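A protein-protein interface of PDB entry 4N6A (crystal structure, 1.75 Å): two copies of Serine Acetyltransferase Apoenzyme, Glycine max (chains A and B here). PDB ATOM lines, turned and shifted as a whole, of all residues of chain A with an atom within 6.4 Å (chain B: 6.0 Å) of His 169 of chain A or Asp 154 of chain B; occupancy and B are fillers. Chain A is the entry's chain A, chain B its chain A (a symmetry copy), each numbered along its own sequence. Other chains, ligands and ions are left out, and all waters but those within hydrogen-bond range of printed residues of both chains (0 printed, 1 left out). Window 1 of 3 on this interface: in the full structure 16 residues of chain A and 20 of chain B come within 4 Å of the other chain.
Printed residues of chain B that touch a printed residue of chain A: Asp 154, Gly 172 and Val 174. Hydrophobic or aromatic side chains of chain B that line the printed part of chain A: Val 174. Along chain B the printed residues that touch a printed residue of chain A span positions 154 to 174. Of the 11 printed residues of chain A, 3 touch a printed residue of chain B. Hydrophobic or aromatic side chains of chain A within 4 Å of the printed part of chain B: His 169, His 189 and His 190. Among the printed residues, no Asp or Glu carboxylate lies within 4 Å of a Lys or Arg side-chain nitrogen of the other chain.
The backbone NH (N) of Gly 172 of chain B lies within hydrogen-bond range of the backbone carbonyl oxygen (O) of Ala 152 of chain B, 2.9 Å away. N of Val 175 of chain B is in hydrogen-bond range of O of Asp 154 of chain B, 2.8 Å away. The backbone carbonyl oxygen (O) of His 169 of chain A is in hydrogen-bond range of a ring nitrogen (ND1) of His 189 of chain A. The backbone carbonyl oxygen (O) of Asp 168 of chain A lies within hydrogen-bond range of the backbone NH (N) of His 189 of chain A, 3.0 Å away. A ring nitrogen (ND1) of His 169 of chain A is in hydrogen-bond range of the side-chain carboxylate of Asp 168 of chain A (2.7 Å). The backbone carbonyl oxygen of Val 173 of chain B sits at hydrogen-bond distance from the backbone NH of Asp 154 of chain B (2.9 Å).
Asp 154 of chain B touches His 169 of chain A. Val 174 of chain B touches His 169 of chain A. His 189 of chain A touches Gly 172 of chain B (NE2 to O, 3.5 Å). His 189 of chain A touches Val 174 of chain B. O of Gly 172 of chain B touches NE2 of His 190 of chain A, at 3.8 Å.
Positions printed for both chains: 172 and 173. Of the 5 pairs that touch across the chains among the printed residues, none has its exchanged pair printed and touching as well.
Asp 154 of chain B touches just one residue of chain A: His 169 (3.2 Å). Printed residues of chain B within 4 Å of His 190 of chain A: Gly 172 (3.8 Å). Of the printed residues of chain B, His 189 of chain A touches Gly 172 (3.5 Å) and Val 174 (3.3 Å). Of the printed residues of chain A, Gly 172 of chain B touches His 189 and His 190. Of the printed residues of chain A, Val 174 of chain B touches His 169 and His 189. Thr 171 of chain A touches none of the printed residues of chain B. Ile 155 of chain B touches none of the printed residues of chain A.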
ATOM      1  N   PHE A 167     -12.867 -29.163  -6.618  1.00  0.00           N
ATOM      2  CA  PHE A 167     -13.862 -28.259  -7.212  1.00  0.00           C
ATOM      3  C   PHE A 167     -15.164 -28.985  -7.528  1.00  0.00           C
ATOM      4  O   PHE A 167     -15.410 -29.298  -8.690  1.00  0.00           O
ATOM      5  CB  PHE A 167     -13.352 -27.650  -8.530  1.00  0.00           C
ATOM      6  CG  PHE A 167     -12.611 -26.350  -8.382  1.00  0.00           C
ATOM      7  CD1 PHE A 167     -13.252 -25.210  -7.951  1.00  0.00           C
ATOM      8  CD2 PHE A 167     -11.269 -26.272  -8.727  1.00  0.00           C
ATOM      9  CE1 PHE A 167     -12.562 -24.021  -7.824  1.00  0.00           C
ATOM     10  CE2 PHE A 167     -10.579 -25.096  -8.612  1.00  0.00           C
ATOM     11  CZ  PHE A 167     -11.219 -23.965  -8.160  1.00  0.00           C
ATOM     12  N   ASP A 168     -15.996 -29.223  -6.519  1.00  0.00           N
ATOM     13  CA  ASP A 168     -17.216 -30.019  -6.655  1.00  0.00           C
ATOM     14  C   ASP A 168     -18.387 -29.263  -7.292  1.00  0.00           C
ATOM     15  O   ASP A 168     -18.852 -28.248  -6.765  1.00  0.00           O
ATOM     16  CB  ASP A 168     -17.637 -30.547  -5.283  1.00  0.00           C
ATOM     17  CG  ASP A 168     -18.946 -31.301  -5.328  1.00  0.00           C
ATOM     18  OD1 ASP A 168     -18.999 -32.361  -5.989  1.00  0.00           O
ATOM     19  OD2 ASP A 168     -19.918 -30.840  -4.690  1.00  0.00           O
ATOM     20  N   HIS A 169     -18.877 -29.793  -8.415  1.00  0.00           N
ATOM     21  CA  HIS A 169     -19.916 -29.137  -9.222  1.00  0.00           C
ATOM     22  C   HIS A 169     -19.474 -27.718  -9.544  1.00  0.00           C
ATOM     23  O   HIS A 169     -20.074 -26.733  -9.104  1.00  0.00           O
ATOM     24  CB  HIS A 169     -21.277 -29.141  -8.512  1.00  0.00           C
ATOM     25  CG  HIS A 169     -21.741 -30.505  -8.105  1.00  0.00           C
ATOM     26  ND1 HIS A 169     -21.663 -30.960  -6.808  1.00  0.00           N
ATOM     27  CD2 HIS A 169     -22.276 -31.519  -8.827  1.00  0.00           C
ATOM     28  CE1 HIS A 169     -22.138 -32.191  -6.744  1.00  0.00           C
ATOM     29  NE2 HIS A 169     -22.517 -32.554  -7.955  1.00  0.00           N
ATOM     30  N   ALA A 170     -18.409 -27.642 -10.332  1.00  0.00           N
ATOM     31  CA  ALA A 170     -17.663 -26.414 -10.545  1.00  0.00           C
ATOM     32  C   ALA A 170     -18.439 -25.335 -11.280  1.00  0.00           C
ATOM     33  O   ALA A 170     -18.011 -24.184 -11.314  1.00  0.00           O
ATOM     34  CB  ALA A 170     -16.373 -26.723 -11.303  1.00  0.00           C
ATOM     35  N   THR A 171     -19.556 -25.701 -11.890  1.00  0.00           N
ATOM     36  CA  THR A 171     -20.314 -24.733 -12.669  1.00  0.00           C
ATOM     37  C   THR A 171     -20.591 -23.491 -11.830  1.00  0.00           C
ATOM     38  O   THR A 171     -21.045 -23.584 -10.689  1.00  0.00           O
ATOM     39  CB  THR A 171     -21.638 -25.331 -13.199  1.00  0.00           C
ATOM     40  OG1 THR A 171     -21.366 -26.539 -13.925  1.00  0.00           O
ATOM     41  CG2 THR A 171     -22.357 -24.342 -14.102  1.00  0.00           C
ATOM     42  N   GLY A 172     -20.251 -22.336 -12.385  1.00  0.00           N
ATOM     43  CA  GLY A 172     -20.564 -21.071 -11.755  1.00  0.00           C
ATOM     44  C   GLY A 172     -19.598 -20.668 -10.663  1.00  0.00           C
ATOM     45  O   GLY A 172     -19.857 -19.707  -9.938  1.00  0.00           O
ATOM     46  N   VAL A 173     -18.484 -21.383 -10.541  1.00  0.00           N
ATOM     47  CA  VAL A 173     -17.416 -20.936  -9.637  1.00  0.00           C
ATOM     48  C   VAL A 173     -16.793 -19.643 -10.155  1.00  0.00           C
ATOM     49  O   VAL A 173     -16.470 -19.531 -11.340  1.00  0.00           O
ATOM     50  CB  VAL A 173     -16.309 -22.011  -9.468  1.00  0.00           C
ATOM     51  CG1 VAL A 173     -15.048 -21.410  -8.879  1.00  0.00           C
ATOM     52  CG2 VAL A 173     -16.790 -23.103  -8.551  1.00  0.00           C
ATOM     53  N   ILE A 187     -13.709 -26.412  -2.862  1.00  0.00           N
ATOM     54  CA  ILE A 187     -14.610 -25.347  -3.264  1.00  0.00           C
ATOM     55  C   ILE A 187     -15.818 -25.969  -3.951  1.00  0.00           C
ATOM     56  O   ILE A 187     -15.701 -26.566  -5.020  1.00  0.00           O
ATOM     57  CB  ILE A 187     -13.925 -24.345  -4.190  1.00  0.00           C
ATOM     58  CG1 ILE A 187     -12.659 -23.786  -3.527  1.00  0.00           C
ATOM     59  CG2 ILE A 187     -14.880 -23.209  -4.536  1.00  0.00           C
ATOM     60  CD1 ILE A 187     -11.534 -23.494  -4.508  1.00  0.00           C
ATOM     61  N   LEU A 188     -16.972 -25.859  -3.309  1.00  0.00           N
ATOM     62  CA  LEU A 188     -18.146 -26.549  -3.808  1.00  0.00           C
ATOM     63  C   LEU A 188     -18.914 -25.671  -4.795  1.00  0.00           C
ATOM     64  O   LEU A 188     -18.422 -24.635  -5.254  1.00  0.00           O
ATOM     65  CB  LEU A 188     -19.037 -26.997  -2.646  1.00  0.00           C
ATOM     66  CG  LEU A 188     -18.343 -27.853  -1.568  1.00  0.00           C
ATOM     67  CD1 LEU A 188     -19.355 -28.559  -0.670  1.00  0.00           C
ATOM     68  CD2 LEU A 188     -17.371 -28.855  -2.163  1.00  0.00           C
ATOM     69  N   HIS A 189     -20.116 -26.111  -5.132  1.00  0.00           N
ATOM     70  CA  HIS A 189     -20.895 -25.506  -6.198  1.00  0.00           C
ATOM     71  C   HIS A 189     -21.295 -24.057  -5.921  1.00  0.00           C
ATOM     72  O   HIS A 189     -21.734 -23.732  -4.823  1.00  0.00           O
ATOM     73  CB  HIS A 189     -22.140 -26.354  -6.427  1.00  0.00           C
ATOM     74  CG  HIS A 189     -23.027 -25.832  -7.505  1.00  0.00           C
ATOM     75  ND1 HIS A 189     -22.558 -25.527  -8.765  1.00  0.00           N
ATOM     76  CD2 HIS A 189     -24.348 -25.546  -7.513  1.00  0.00           C
ATOM     77  CE1 HIS A 189     -23.557 -25.084  -9.507  1.00  0.00           C
ATOM     78  NE2 HIS A 189     -24.654 -25.083  -8.770  1.00  0.00           N
ATOM     79  N   HIS A 190     -21.135 -23.196  -6.932  1.00  0.00           N
ATOM     80  CA  HIS A 190     -21.589 -21.800  -6.881  1.00  0.00           C
ATOM     81  C   HIS A 190     -20.916 -20.979  -5.799  1.00  0.00           C
ATOM     82  O   HIS A 190     -21.557 -20.146  -5.150  1.00  0.00           O
ATOM     83  CB  HIS A 190     -23.105 -21.728  -6.680  1.00  0.00           C
ATOM     84  CG  HIS A 190     -23.889 -21.875  -7.946  1.00  0.00           C
ATOM     85  ND1 HIS A 190     -23.292 -21.942  -9.187  1.00  0.00           N
ATOM     86  CD2 HIS A 190     -25.222 -21.942  -8.164  1.00  0.00           C
ATOM     87  CE1 HIS A 190     -24.225 -22.061 -10.114  1.00  0.00           C
ATOM     88  NE2 HIS A 190     -25.405 -22.065  -9.520  1.00  0.00           N
ATOM     89  N   HIS B 144     -24.165 -37.355 -19.922  1.00  0.00           N
ATOM     90  CA  HIS B 144     -24.379 -36.422 -18.810  1.00  0.00           C
ATOM     91  C   HIS B 144     -23.484 -35.189 -18.907  1.00  0.00           C
ATOM     92  O   HIS B 144     -23.925 -34.062 -18.670  1.00  0.00           O
ATOM     93  CB  HIS B 144     -24.149 -37.166 -17.484  1.00  0.00           C
ATOM     94  CG  HIS B 144     -23.928 -36.266 -16.311  1.00  0.00           C
ATOM     95  ND1 HIS B 144     -22.694 -36.098 -15.725  1.00  0.00           N
ATOM     96  CD2 HIS B 144     -24.790 -35.499 -15.604  1.00  0.00           C
ATOM     97  CE1 HIS B 144     -22.803 -35.262 -14.708  1.00  0.00           C
ATOM     98  NE2 HIS B 144     -24.065 -34.881 -14.616  1.00  0.00           N
ATOM     99  N   ILE B 147     -24.860 -32.892 -21.596  1.00  0.00           N
ATOM    100  CA  ILE B 147     -26.094 -32.236 -21.152  1.00  0.00           C
ATOM    101  C   ILE B 147     -25.750 -31.042 -20.271  1.00  0.00           C
ATOM    102  O   ILE B 147     -26.343 -29.967 -20.404  1.00  0.00           O
ATOM    103  CB  ILE B 147     -27.007 -33.208 -20.385  1.00  0.00           C
ATOM    104  CG1 ILE B 147     -27.490 -34.324 -21.323  1.00  0.00           C
ATOM    105  CG2 ILE B 147     -28.180 -32.462 -19.694  1.00  0.00           C
ATOM    106  CD1 ILE B 147     -28.077 -35.501 -20.585  1.00  0.00           C
ATOM    107  N   ALA B 148     -24.768 -31.234 -19.395  1.00  0.00           N
ATOM    108  CA  ALA B 148     -24.287 -30.158 -18.524  1.00  0.00           C
ATOM    109  C   ALA B 148     -23.661 -29.028 -19.349  1.00  0.00           C
ATOM    110  O   ALA B 148     -23.989 -27.853 -19.150  1.00  0.00           O
ATOM    111  CB  ALA B 148     -23.276 -30.706 -17.514  1.00  0.00           C
ATOM    112  N   ALA B 152     -26.796 -26.499 -19.337  1.00  0.00           N
ATOM    113  CA  ALA B 152     -26.508 -26.028 -17.987  1.00  0.00           C
ATOM    114  C   ALA B 152     -27.399 -26.733 -16.962  1.00  0.00           C
ATOM    115  O   ALA B 152     -27.946 -26.122 -16.045  1.00  0.00           O
ATOM    116  CB  ALA B 152     -26.674 -24.534 -17.916  1.00  0.00           C
ATOM    117  N   VAL B 153     -27.555 -28.036 -17.149  1.00  0.00           N
ATOM    118  CA  VAL B 153     -28.336 -28.854 -16.252  1.00  0.00           C
ATOM    119  C   VAL B 153     -27.483 -30.034 -15.831  1.00  0.00           C
ATOM    120  O   VAL B 153     -27.070 -30.828 -16.670  1.00  0.00           O
ATOM    121  CB  VAL B 153     -29.637 -29.334 -16.903  1.00  0.00           C
ATOM    122  CG1 VAL B 153     -30.332 -30.319 -16.021  1.00  0.00           C
ATOM    123  CG2 VAL B 153     -30.547 -28.156 -17.210  1.00  0.00           C
ATOM    124  N   ASP B 154     -27.190 -30.124 -14.536  1.00  0.00           N
ATOM    125  CA  ASP B 154     -26.293 -31.156 -14.036  1.00  0.00           C
ATOM    126  C   ASP B 154     -27.081 -32.108 -13.156  1.00  0.00           C
ATOM    127  O   ASP B 154     -27.183 -31.911 -11.942  1.00  0.00           O
ATOM    128  CB  ASP B 154     -25.126 -30.525 -13.277  1.00  0.00           C
ATOM    129  CG  ASP B 154     -24.231 -31.554 -12.584  1.00  0.00           C
ATOM    130  OD1 ASP B 154     -24.364 -32.769 -12.843  1.00  0.00           O
ATOM    131  OD2 ASP B 154     -23.385 -31.133 -11.773  1.00  0.00           O
ATOM    132  N   ILE B 155     -27.638 -33.133 -13.797  1.00  0.00           N
ATOM    133  CA  ILE B 155     -28.392 -34.184 -13.121  1.00  0.00           C
ATOM    134  C   ILE B 155     -27.625 -35.493 -13.256  1.00  0.00           C
ATOM    135  O   ILE B 155     -27.463 -35.987 -14.369  1.00  0.00           O
ATOM    136  CB  ILE B 155     -29.809 -34.369 -13.719  1.00  0.00           C
ATOM    137  CG1 ILE B 155     -30.575 -33.046 -13.766  1.00  0.00           C
ATOM    138  CG2 ILE B 155     -30.589 -35.407 -12.934  1.00  0.00           C
ATOM    139  CD1 ILE B 155     -31.906 -33.145 -14.498  1.00  0.00           C
ATOM    140  N   HIS B 156     -27.148 -36.054 -12.150  1.00  0.00           N
ATOM    141  CA  HIS B 156     -26.359 -37.287 -12.242  1.00  0.00           C
ATOM    142  C   HIS B 156     -27.207 -38.410 -12.850  1.00  0.00           C
ATOM    143  O   HIS B 156     -28.382 -38.527 -12.538  1.00  0.00           O
ATOM    144  CB  HIS B 156     -25.830 -37.703 -10.864  1.00  0.00           C
ATOM    145  CG  HIS B 156     -24.807 -38.793 -10.924  1.00  0.00           C
ATOM    146  ND1 HIS B 156     -25.145 -40.121 -11.071  1.00  0.00           N
ATOM    147  CD2 HIS B 156     -23.454 -38.748 -10.907  1.00  0.00           C
ATOM    148  CE1 HIS B 156     -24.043 -40.849 -11.119  1.00  0.00           C
ATOM    149  NE2 HIS B 156     -23.003 -40.040 -11.024  1.00  0.00           N
ATOM    150  N   GLY B 172     -27.676 -23.868 -14.247  1.00  0.00           N
ATOM    151  CA  GLY B 172     -27.079 -24.016 -12.938  1.00  0.00           C
ATOM    152  C   GLY B 172     -27.842 -24.932 -12.008  1.00  0.00           C
ATOM    153  O   GLY B 172     -27.532 -24.999 -10.818  1.00  0.00           O
ATOM    154  N   VAL B 173     -28.831 -25.648 -12.536  1.00  0.00           N
ATOM    155  CA  VAL B 173     -29.488 -26.697 -11.743  1.00  0.00           C
ATOM    156  C   VAL B 173     -28.514 -27.837 -11.466  1.00  0.00           C
ATOM    157  O   VAL B 173     -27.824 -28.309 -12.374  1.00  0.00           O
ATOM    158  CB  VAL B 173     -30.751 -27.256 -12.451  1.00  0.00           C
ATOM    159  CG1 VAL B 173     -31.179 -28.577 -11.843  1.00  0.00           C
ATOM    160  CG2 VAL B 173     -31.888 -26.279 -12.320  1.00  0.00           C
ATOM    161  N   VAL B 174     -28.448 -28.254 -10.204  1.00  0.00           N
ATOM    162  CA  VAL B 174     -27.646 -29.406  -9.799  1.00  0.00           C
ATOM    163  C   VAL B 174     -28.508 -30.397  -9.035  1.00  0.00           C
ATOM    164  O   VAL B 174     -29.163 -30.041  -8.047  1.00  0.00           O
ATOM    165  CB  VAL B 174     -26.449 -28.998  -8.917  1.00  0.00           C
ATOM    166  CG1 VAL B 174     -25.787 -30.228  -8.322  1.00  0.00           C
ATOM    167  CG2 VAL B 174     -25.444 -28.192  -9.725  1.00  0.00           C
ATOM    168  N   VAL B 175     -28.522 -31.635  -9.515  1.00  0.00           N
ATOM    169  CA  VAL B 175     -29.243 -32.726  -8.852  1.00  0.00           C
ATOM    170  C   VAL B 175     -28.263 -33.875  -8.640  1.00  0.00           C
ATOM    171  O   VAL B 175     -27.758 -34.456  -9.596  1.00  0.00           O
ATOM    172  CB  VAL B 175     -30.464 -33.218  -9.666  1.00  0.00           C
ATOM    173  CG1 VAL B 175     -31.113 -34.418  -8.979  1.00  0.00           C
ATOM    174  CG2 VAL B 175     -31.481 -32.103  -9.852  1.00  0.00           C
ATOM    175  N   GLY B 176     -28.004 -34.201  -7.380  1.00  0.00           N
ATOM    176  CA  GLY B 176     -26.956 -35.142  -7.054  1.00  0.00           C
ATOM    177  C   GLY B 176     -27.295 -36.600  -7.274  1.00  0.00           C
ATOM    178  O   GLY B 176     -28.461 -36.971  -7.449  1.00  0.00           O
ATOM    179  N   GLY B 194     -28.251 -31.405  -3.445  1.00  0.00           N
ATOM    180  CA  GLY B 194     -26.912 -31.953  -3.317  1.00  0.00           C
ATOM    181  C   GLY B 194     -26.509 -32.286  -1.891  1.00  0.00           C
ATOM    182  O   GLY B 194     -27.351 -32.586  -1.048  1.00  0.00           O
ATOM    183  N   GLY B 195     -25.209 -32.224  -1.618  1.00  0.00           N
ATOM    184  CA  GLY B 195     -24.685 -32.718  -0.357  1.00  0.00           C
ATOM    185  C   GLY B 195     -23.781 -31.777   0.418  1.00  0.00           C
ATOM    186  O   GLY B 195     -23.474 -30.673  -0.033  1.00  0.00           O
ATOM    187  N   HIS B 204     -28.140 -37.165  -0.732  1.00  0.00           N
ATOM    188  CA  HIS B 204     -28.896 -36.178  -1.497  1.00  0.00           C
ATOM    189  C   HIS B 204     -30.407 -36.279  -1.212  1.00  0.00           C
ATOM    190  O   HIS B 204     -30.904 -37.339  -0.839  1.00  0.00           O
ATOM    191  CB  HIS B 204     -28.595 -36.345  -2.992  1.00  0.00           C
ATOM    192  CG  HIS B 204     -27.138 -36.207  -3.324  1.00  0.00           C
ATOM    193  ND1 HIS B 204     -26.462 -37.126  -4.101  1.00  0.00           N
ATOM    194  CD2 HIS B 204     -26.230 -35.270  -2.974  1.00  0.00           C
ATOM    195  CE1 HIS B 204     -25.201 -36.751  -4.219  1.00  0.00           C
ATOM    196  NE2 HIS B 204     -25.031 -35.628  -3.547  1.00  0.00           N
